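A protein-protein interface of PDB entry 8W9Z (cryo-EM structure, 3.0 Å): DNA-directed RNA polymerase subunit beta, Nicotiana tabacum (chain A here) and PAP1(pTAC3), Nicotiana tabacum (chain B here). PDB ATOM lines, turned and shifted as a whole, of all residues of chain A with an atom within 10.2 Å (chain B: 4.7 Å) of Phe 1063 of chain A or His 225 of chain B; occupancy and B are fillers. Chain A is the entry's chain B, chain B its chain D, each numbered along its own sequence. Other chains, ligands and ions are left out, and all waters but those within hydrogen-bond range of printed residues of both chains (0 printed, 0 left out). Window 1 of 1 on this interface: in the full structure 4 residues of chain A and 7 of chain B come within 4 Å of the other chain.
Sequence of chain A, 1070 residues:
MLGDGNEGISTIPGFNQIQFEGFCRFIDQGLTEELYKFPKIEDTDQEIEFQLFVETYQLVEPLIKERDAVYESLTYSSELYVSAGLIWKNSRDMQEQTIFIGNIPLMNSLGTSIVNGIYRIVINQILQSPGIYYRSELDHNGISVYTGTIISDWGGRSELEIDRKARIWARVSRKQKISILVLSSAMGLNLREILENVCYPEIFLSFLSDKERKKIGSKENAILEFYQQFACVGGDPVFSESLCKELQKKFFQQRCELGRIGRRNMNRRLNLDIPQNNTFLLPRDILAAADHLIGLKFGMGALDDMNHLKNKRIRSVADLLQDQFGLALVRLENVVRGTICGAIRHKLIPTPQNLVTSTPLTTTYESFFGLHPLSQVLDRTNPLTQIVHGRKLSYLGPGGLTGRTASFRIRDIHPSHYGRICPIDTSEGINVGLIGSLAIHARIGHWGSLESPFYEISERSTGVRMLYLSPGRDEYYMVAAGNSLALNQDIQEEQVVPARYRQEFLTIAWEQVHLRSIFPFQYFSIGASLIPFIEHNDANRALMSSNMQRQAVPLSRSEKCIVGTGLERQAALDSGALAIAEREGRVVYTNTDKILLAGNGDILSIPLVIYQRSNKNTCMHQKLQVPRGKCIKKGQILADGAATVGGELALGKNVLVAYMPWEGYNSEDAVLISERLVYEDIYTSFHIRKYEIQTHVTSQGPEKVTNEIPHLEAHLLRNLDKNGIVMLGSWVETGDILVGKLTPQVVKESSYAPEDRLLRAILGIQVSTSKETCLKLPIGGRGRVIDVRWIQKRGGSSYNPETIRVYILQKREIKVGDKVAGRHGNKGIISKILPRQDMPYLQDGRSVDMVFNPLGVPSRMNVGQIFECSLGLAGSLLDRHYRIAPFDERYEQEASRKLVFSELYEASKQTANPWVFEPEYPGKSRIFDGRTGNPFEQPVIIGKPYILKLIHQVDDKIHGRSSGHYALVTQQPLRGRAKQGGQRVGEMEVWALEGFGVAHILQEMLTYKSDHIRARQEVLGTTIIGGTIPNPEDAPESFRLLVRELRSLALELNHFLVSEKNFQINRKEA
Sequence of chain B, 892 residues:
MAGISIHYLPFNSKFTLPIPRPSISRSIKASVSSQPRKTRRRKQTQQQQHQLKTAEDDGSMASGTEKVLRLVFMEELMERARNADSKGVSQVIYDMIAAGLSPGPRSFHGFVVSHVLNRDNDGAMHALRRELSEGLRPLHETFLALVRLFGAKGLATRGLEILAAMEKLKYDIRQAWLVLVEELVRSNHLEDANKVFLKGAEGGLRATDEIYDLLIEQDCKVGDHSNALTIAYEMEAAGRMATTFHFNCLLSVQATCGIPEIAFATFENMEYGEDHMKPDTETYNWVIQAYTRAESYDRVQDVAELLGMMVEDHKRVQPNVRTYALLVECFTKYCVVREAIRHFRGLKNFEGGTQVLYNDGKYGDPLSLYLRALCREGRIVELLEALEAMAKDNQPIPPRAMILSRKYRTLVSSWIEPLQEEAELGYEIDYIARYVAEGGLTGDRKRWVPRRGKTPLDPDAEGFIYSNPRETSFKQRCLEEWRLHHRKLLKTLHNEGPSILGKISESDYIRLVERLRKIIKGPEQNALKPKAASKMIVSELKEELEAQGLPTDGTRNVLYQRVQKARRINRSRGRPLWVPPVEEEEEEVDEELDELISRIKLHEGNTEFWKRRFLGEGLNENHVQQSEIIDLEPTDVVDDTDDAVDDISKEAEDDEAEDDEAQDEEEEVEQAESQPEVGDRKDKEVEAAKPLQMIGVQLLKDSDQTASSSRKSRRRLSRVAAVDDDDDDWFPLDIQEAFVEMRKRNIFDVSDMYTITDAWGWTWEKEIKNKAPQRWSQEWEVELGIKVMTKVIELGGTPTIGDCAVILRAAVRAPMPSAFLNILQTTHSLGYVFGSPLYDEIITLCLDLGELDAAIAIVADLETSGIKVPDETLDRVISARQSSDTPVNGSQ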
ATOM      1  N   LEU A1057     -16.206 -16.989  22.646  1.00  0.00           N
ATOM      2  CA  LEU A1057     -17.491 -16.418  22.263  1.00  0.00           C
ATOM      3  C   LEU A1057     -17.955 -17.048  20.955  1.00  0.00           C
ATOM      4  O   LEU A1057     -17.330 -16.855  19.908  1.00  0.00           O
ATOM      5  CB  LEU A1057     -17.373 -14.902  22.127  1.00  0.00           C
ATOM      6  CG  LEU A1057     -18.649 -14.058  22.196  1.00  0.00           C
ATOM      7  CD1 LEU A1057     -18.316 -12.645  22.649  1.00  0.00           C
ATOM      8  CD2 LEU A1057     -19.375 -14.023  20.859  1.00  0.00           C
ATOM      9  N   VAL A1058     -19.050 -17.802  21.014  1.00  0.00           N
ATOM     10  CA  VAL A1058     -19.580 -18.524  19.863  1.00  0.00           C
ATOM     11  C   VAL A1058     -20.599 -17.642  19.158  1.00  0.00           C
ATOM     12  O   VAL A1058     -21.463 -17.037  19.806  1.00  0.00           O
ATOM     13  CB  VAL A1058     -20.210 -19.862  20.285  1.00  0.00           C
ATOM     14  CG1 VAL A1058     -20.704 -20.624  19.067  1.00  0.00           C
ATOM     15  CG2 VAL A1058     -19.214 -20.691  21.073  1.00  0.00           C
ATOM     16  N   SER A1059     -20.503 -17.570  17.833  1.00  0.00           N
ATOM     17  CA  SER A1059     -21.432 -16.788  17.031  1.00  0.00           C
ATOM     18  C   SER A1059     -22.581 -17.675  16.572  1.00  0.00           C
ATOM     19  O   SER A1059     -22.360 -18.779  16.064  1.00  0.00           O
ATOM     20  CB  SER A1059     -20.720 -16.174  15.826  1.00  0.00           C
ATOM     21  OG  SER A1059     -20.155 -17.179  15.004  1.00  0.00           O
ATOM     22  N   GLU A1060     -23.809 -17.188  16.754  1.00  0.00           N
ATOM     23  CA  GLU A1060     -24.997 -17.967  16.434  1.00  0.00           C
ATOM     24  C   GLU A1060     -25.382 -17.900  14.962  1.00  0.00           C
ATOM     25  O   GLU A1060     -26.280 -18.639  14.544  1.00  0.00           O
ATOM     26  CB  GLU A1060     -26.180 -17.502  17.288  1.00  0.00           C
ATOM     27  CG  GLU A1060     -26.762 -16.154  16.881  1.00  0.00           C
ATOM     28  CD  GLU A1060     -25.875 -14.985  17.266  1.00  0.00           C
ATOM     29  OE1 GLU A1060     -24.943 -15.182  18.073  1.00  0.00           O
ATOM     30  OE2 GLU A1060     -26.112 -13.868  16.761  1.00  0.00           O
ATOM     31  N   LYS A1061     -24.738 -17.042  14.171  1.00  0.00           N
ATOM     32  CA  LYS A1061     -25.109 -16.918  12.766  1.00  0.00           C
ATOM     33  C   LYS A1061     -24.321 -17.882  11.886  1.00  0.00           C
ATOM     34  O   LYS A1061     -24.909 -18.684  11.152  1.00  0.00           O
ATOM     35  CB  LYS A1061     -24.913 -15.476  12.296  1.00  0.00           C
ATOM     36  CG  LYS A1061     -25.905 -14.494  12.896  1.00  0.00           C
ATOM     37  CD  LYS A1061     -25.732 -13.101  12.314  1.00  0.00           C
ATOM     38  CE  LYS A1061     -26.765 -12.137  12.879  1.00  0.00           C
ATOM     39  NZ  LYS A1061     -26.621 -10.771  12.305  1.00  0.00           N
ATOM     40  N   ASN A1062     -22.992 -17.823  11.946  1.00  0.00           N
ATOM     41  CA  ASN A1062     -22.140 -18.633  11.087  1.00  0.00           C
ATOM     42  C   ASN A1062     -21.550 -19.846  11.793  1.00  0.00           C
ATOM     43  O   ASN A1062     -20.850 -20.636  11.150  1.00  0.00           O
ATOM     44  CB  ASN A1062     -21.013 -17.774  10.504  1.00  0.00           C
ATOM     45  CG  ASN A1062     -20.333 -16.916  11.550  1.00  0.00           C
ATOM     46  OD1 ASN A1062     -20.460 -17.162  12.749  1.00  0.00           O
ATOM     47  ND2 ASN A1062     -19.606 -15.901  11.101  1.00  0.00           N
ATOM     48  N   PHE A1063     -21.806 -20.007  13.093  1.00  0.00           N
ATOM     49  CA  PHE A1063     -21.380 -21.185  13.852  1.00  0.00           C
ATOM     50  C   PHE A1063     -19.860 -21.346  13.836  1.00  0.00           C
ATOM     51  O   PHE A1063     -19.326 -22.385  13.446  1.00  0.00           O
ATOM     52  CB  PHE A1063     -22.068 -22.451  13.333  1.00  0.00           C
ATOM     53  CG  PHE A1063     -23.551 -22.468  13.547  1.00  0.00           C
ATOM     54  CD1 PHE A1063     -24.127 -21.716  14.556  1.00  0.00           C
ATOM     55  CD2 PHE A1063     -24.370 -23.237  12.740  1.00  0.00           C
ATOM     56  CE1 PHE A1063     -25.492 -21.729  14.754  1.00  0.00           C
ATOM     57  CE2 PHE A1063     -25.735 -23.254  12.933  1.00  0.00           C
ATOM     58  CZ  PHE A1063     -26.296 -22.499  13.942  1.00  0.00           C
ATOM     59  N   GLN A1064     -19.162 -20.301  14.269  1.00  0.00           N
ATOM     60  CA  GLN A1064     -17.714 -20.334  14.393  1.00  0.00           C
ATOM     61  C   GLN A1064     -17.318 -19.896  15.795  1.00  0.00           C
ATOM     62  O   GLN A1064     -18.001 -19.085  16.427  1.00  0.00           O
ATOM     63  CB  GLN A1064     -17.031 -19.440  13.348  1.00  0.00           C
ATOM     64  CG  GLN A1064     -17.358 -17.964  13.474  1.00  0.00           C
ATOM     65  CD  GLN A1064     -16.632 -17.119  12.448  1.00  0.00           C
ATOM     66  OE1 GLN A1064     -15.907 -17.640  11.600  1.00  0.00           O
ATOM     67  NE2 GLN A1064     -16.822 -15.806  12.520  1.00  0.00           N
ATOM     68  N   ILE A1065     -16.210 -20.446  16.279  1.00  0.00           N
ATOM     69  CA  ILE A1065     -15.709 -20.167  17.619  1.00  0.00           C
ATOM     70  C   ILE A1065     -14.579 -19.153  17.515  1.00  0.00           C
ATOM     71  O   ILE A1065     -13.635 -19.343  16.738  1.00  0.00           O
ATOM     72  CB  ILE A1065     -15.236 -21.453  18.317  1.00  0.00           C
ATOM     73  CG1 ILE A1065     -16.393 -22.449  18.430  1.00  0.00           C
ATOM     74  CG2 ILE A1065     -14.666 -21.136  19.691  1.00  0.00           C
ATOM     75  CD1 ILE A1065     -16.030 -23.732  19.139  1.00  0.00           C
ATOM     76  N   ASN A1066     -14.674 -18.080  18.295  1.00  0.00           N
ATOM     77  CA  ASN A1066     -13.684 -17.010  18.296  1.00  0.00           C
ATOM     78  C   ASN A1066     -13.143 -16.839  19.707  1.00  0.00           C
ATOM     79  O   ASN A1066     -13.888 -16.467  20.620  1.00  0.00           O
ATOM     80  CB  ASN A1066     -14.291 -15.700  17.789  1.00  0.00           C
ATOM     81  CG  ASN A1066     -14.850 -15.821  16.387  1.00  0.00           C
ATOM     82  OD1 ASN A1066     -14.378 -16.628  15.586  1.00  0.00           O
ATOM     83  ND2 ASN A1066     -15.862 -15.017  16.082  1.00  0.00           N
ATOM     84  N   GLY B 223     -27.868 -24.475   3.390  1.00  0.00           N
ATOM     85  CA  GLY B 223     -26.994 -24.563   4.543  1.00  0.00           C
ATOM     86  C   GLY B 223     -26.600 -23.210   5.097  1.00  0.00           C
ATOM     87  O   GLY B 223     -25.661 -23.106   5.891  1.00  0.00           O
ATOM     88  N   ASP B 224     -27.315 -22.165   4.688  1.00  0.00           N
ATOM     89  CA  ASP B 224     -27.026 -20.802   5.117  1.00  0.00           C
ATOM     90  C   ASP B 224     -27.877 -20.489   6.342  1.00  0.00           C
ATOM     91  O   ASP B 224     -29.106 -20.391   6.246  1.00  0.00           O
ATOM     92  CB  ASP B 224     -27.299 -19.816   3.983  1.00  0.00           C
ATOM     93  CG  ASP B 224     -26.616 -18.478   4.192  1.00  0.00           C
ATOM     94  OD1 ASP B 224     -26.503 -18.033   5.354  1.00  0.00           O
ATOM     95  OD2 ASP B 224     -26.187 -17.871   3.189  1.00  0.00           O
ATOM     96  N   HIS B 225     -27.227 -20.333   7.493  1.00  0.00           N
ATOM     97  CA  HIS B 225     -27.936 -20.053   8.734  1.00  0.00           C
ATOM     98  C   HIS B 225     -28.030 -18.565   9.041  1.00  0.00           C
ATOM     99  O   HIS B 225     -29.015 -18.130   9.648  1.00  0.00           O
ATOM    100  CB  HIS B 225     -27.256 -20.772   9.903  1.00  0.00           C
ATOM    101  CG  HIS B 225     -28.009 -20.675  11.194  1.00  0.00           C
ATOM    102  ND1 HIS B 225     -27.984 -19.549  11.988  1.00  0.00           N
ATOM    103  CD2 HIS B 225     -28.802 -21.567  11.831  1.00  0.00           C
ATOM    104  CE1 HIS B 225     -28.733 -19.750  13.056  1.00  0.00           C
ATOM    105  NE2 HIS B 225     -29.241 -20.967  12.986  1.00  0.00           N
ATOM    106  N   SER B 226     -27.034 -17.776   8.633  1.00  0.00           N
ATOM    107  CA  SER B 226     -27.028 -16.353   8.959  1.00  0.00           C
ATOM    108  C   SER B 226     -28.187 -15.627   8.287  1.00  0.00           C
ATOM    109  O   SER B 226     -28.939 -14.894   8.941  1.00  0.00           O
ATOM    110  CB  SER B 226     -25.694 -15.730   8.552  1.00  0.00           C
ATOM    111  OG  SER B 226     -24.607 -16.403   9.161  1.00  0.00           O
ATOM    112  N   ASN B 227     -28.345 -15.820   6.976  1.00  0.00           N
ATOM    113  CA  ASN B 227     -29.425 -15.152   6.260  1.00  0.00           C
ATOM    114  C   ASN B 227     -30.788 -15.659   6.715  1.00  0.00           C
ATOM    115  O   ASN B 227     -31.745 -14.882   6.805  1.00  0.00           O
ATOM    116  CB  ASN B 227     -29.253 -15.341   4.754  1.00  0.00           C
ATOM    117  CG  ASN B 227     -28.032 -14.626   4.215  1.00  0.00           C
ATOM    118  OD1 ASN B 227     -27.142 -15.243   3.631  1.00  0.00           O
ATOM    119  ND2 ASN B 227     -27.981 -13.313   4.411  1.00  0.00           N
ATOM    120  N   ALA B 228     -30.892 -16.955   7.016  1.00  0.00           N
ATOM    121  CA  ALA B 228     -32.152 -17.495   7.517  1.00  0.00           C
ATOM    122  C   ALA B 228     -32.528 -16.867   8.853  1.00  0.00           C
ATOM    123  O   ALA B 228     -33.685 -16.486   9.065  1.00  0.00           O
ATOM    124  CB  ALA B 228     -32.062 -19.014   7.644  1.00  0.00           C
ATOM    125  N   LEU B 229     -31.561 -16.740   9.764  1.00  0.00           N
ATOM    126  CA  LEU B 229     -31.846 -16.135  11.060  1.00  0.00           C
ATOM    127  C   LEU B 229     -32.177 -14.654  10.918  1.00  0.00           C
ATOM    128  O   LEU B 229     -33.050 -14.137  11.625  1.00  0.00           O
ATOM    129  CB  LEU B 229     -30.661 -16.338  12.003  1.00  0.00           C
ATOM    130  CG  LEU B 229     -30.914 -16.084  13.489  1.00  0.00           C
ATOM    131  CD1 LEU B 229     -32.034 -16.973  13.996  1.00  0.00           C
ATOM    132  CD2 LEU B 229     -29.645 -16.314  14.291  1.00  0.00           C
ATOM    133  N   LEU B 250     -34.388 -24.025  10.953  1.00  0.00           N
ATOM    134  CA  LEU B 250     -33.205 -23.536  11.588  1.00  0.00           C
ATOM    135  C   LEU B 250     -32.496 -24.647  12.355  1.00  0.00           C
ATOM    136  O   LEU B 250     -31.257 -24.698  12.383  1.00  0.00           O
ATOM    137  CB  LEU B 250     -33.496 -22.303  12.399  1.00  0.00           C
ATOM    138  CG  LEU B 250     -33.462 -20.887  11.846  1.00  0.00           C
ATOM    139  CD1 LEU B 250     -34.242 -20.732  10.554  1.00  0.00           C
ATOM    140  CD2 LEU B 250     -34.023 -19.969  12.909  1.00  0.00           C
ATOM    141  N   VAL B 253     -30.325 -26.720  10.135  1.00  0.00           N
ATOM    142  CA  VAL B 253     -28.934 -26.243   9.948  1.00  0.00           C
ATOM    143  C   VAL B 253     -28.072 -26.295  11.193  1.00  0.00           C
ATOM    144  O   VAL B 253     -26.913 -26.554  11.085  1.00  0.00           O
ATOM    145  CB  VAL B 253     -28.759 -24.871   9.384  1.00  0.00           C
ATOM    146  N   GLN B 254     -28.609 -26.010  12.362  1.00  0.00           N
ATOM    147  CA  GLN B 254     -27.869 -26.134  13.613  1.00  0.00           C
ATOM    148  C   GLN B 254     -27.389 -27.521  14.034  1.00  0.00           C
ATOM    149  O   GLN B 254     -26.338 -27.627  14.655  1.00  0.00           O
ATOM    150  CB  GLN B 254     -28.681 -25.546  14.731  1.00  0.00           C
ATOM    151  CG  GLN B 254     -29.050 -24.089  14.614  1.00  0.00           C
ATOM    152  CD  GLN B 254     -29.919 -23.629  15.752  1.00  0.00           C
ATOM    153  OE1 GLN B 254     -30.635 -24.419  16.353  1.00  0.00           O
ATOM    154  NE2 GLN B 254     -29.870 -22.350  16.052  1.00  0.00           N
ATOM    155  N   CYS B 257     -23.684 -28.553  13.393  1.00  0.00           N
ATOM    156  CA  CYS B 257     -22.574 -27.707  13.820  1.00  0.00           C
ATOM    157  C   CYS B 257     -21.569 -28.476  14.669  1.00  0.00           C
ATOM    158  O   CYS B 257     -20.358 -28.273  14.537  1.00  0.00           O
ATOM    159  CB  CYS B 257     -23.103 -26.499  14.591  1.00  0.00           C
ATOM    160  SG  CYS B 257     -21.818 -25.452  15.310  1.00  0.00           S
ATOM    161  N   ILE B 262     -26.513 -25.242  21.066  1.00  0.00           N
ATOM    162  CA  ILE B 262     -27.210 -24.306  20.195  1.00  0.00           C
ATOM    163  C   ILE B 262     -28.529 -24.880  19.697  1.00  0.00           C
ATOM    164  O   ILE B 262     -29.440 -24.119  19.351  1.00  0.00           O
ATOM    165  CB  ILE B 262     -26.318 -23.890  19.011  1.00  0.00           C
ATOM    166  CG1 ILE B 262     -26.046 -25.082  18.093  1.00  0.00           C
ATOM    167  CG2 ILE B 262     -25.010 -23.300  19.511  1.00  0.00           C
ATOM    168  CD1 ILE B 262     -25.253 -24.726  16.860  1.00  0.00           C
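The backbone carbonyl oxygen of Glu 1060 of chain A lies close to a ring nitrogen (ND1) of His 225 of chain B, at 3.2 Å.
The backbone carbonyl oxygen (O) of Lys 1061 of chain A is in hydrogen-bond range of a ring nitrogen (ND1) of His 225 of chain B, at 3.3 Å.
The side-chain hydroxyl of Ser 226 of chain B sits at hydrogen-bond distance from the backbone carbonyl oxygen of Lys 1061 of chain A, 3.0 Å away.
Among the printed residues, merely in contact across the chains: Phe 1063 of chain A with Gln 254 of chain B (3.3 Å), Phe 1063 of chain A with His 225 of chain B (3.4 Å), Asn 1062 of chain A with Ser 226 of chain B (3.5 Å), Phe 1063 of chain A with Cys 257 of chain B (3.6 Å), Phe 1063 of chain A with Ile 262 of chain B (3.7 Å), Glu 1060 of chain A with Leu 229 of chain B (3.9 Å) and Phe 1063 of chain A with Val 253 of chain B (3.96 Å).
Of the printed residues of chain B, Glu 1060 of chain A touches His 225 (3.1 Å) and Leu 229 (3.9 Å).
Printed residues of chain B within 4 Å of Lys 1061 of chain A: His 225 (3.3 Å) and Ser 226 (3.0 Å).
Printed residues of chain B within 4 Å of Asn 1062 of chain A: Ser 226.
Phe 1063 of chain A touches just these residues of chain B: His 225 (3.4 Å), Val 253 (3.96 Å), Gln 254 (3.3 Å), Cys 257 (3.6 Å) and Ile 262 (3.7 Å).
Of chain A, only Glu 1060 (3.1 Å), Lys 1061 (3.3 Å) and Phe 1063 (3.4 Å) come within 4 Å of His 225 of chain B.
Ser 226 of chain B touches two residues of chain A.
No residue of chain A comes within 4 Å of Ala 228 of chain B.
Of chain A, only Glu 1060 comes within 4 Å of Leu 229 of chain B.
Gln 254 of chain B touches one residue of chain A.
Printed residues of chain A within 4 Å of Cys 257 of chain B: Phe 1063.
Printed residues of chain A within 4 Å of Ile 262 of chain B: Phe 1063 (3.7 Å).
Of the 10 printed residues of chain A, 4 touch a printed residue of chain B.
Hydrophobic or aromatic side chains of chain A within 4 Å of the printed part of chain B: Phe 1063.
Printed residues of chain B that touch a printed residue of chain A: His 225, Ser 226, Leu 229, Val 253, Gln 254, Cys 257 and Ile 262.
Among the printed residues, 10 pairs touch across the chains.
NE2 of Gln 1064 of chain A lies close to ND2 of Asn 1062 of chain A (3.1 Å).
The backbone NH of Ser 226 of chain B lies within hydrogen-bond range of the side-chain carboxylate of Asp 224 of chain B (3.3 Å).
A ring nitrogen (NE2) of His 225 of chain B is in hydrogen-bond range of the side-chain amide nitrogen (NE2) of Gln 254 of chain B (3.4 Å).
The side-chain amide oxygen (OE1) of Gln 254 of chain B sits close to the backbone carbonyl oxygen (O) of Ile 262 of chain B (3.2 Å).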
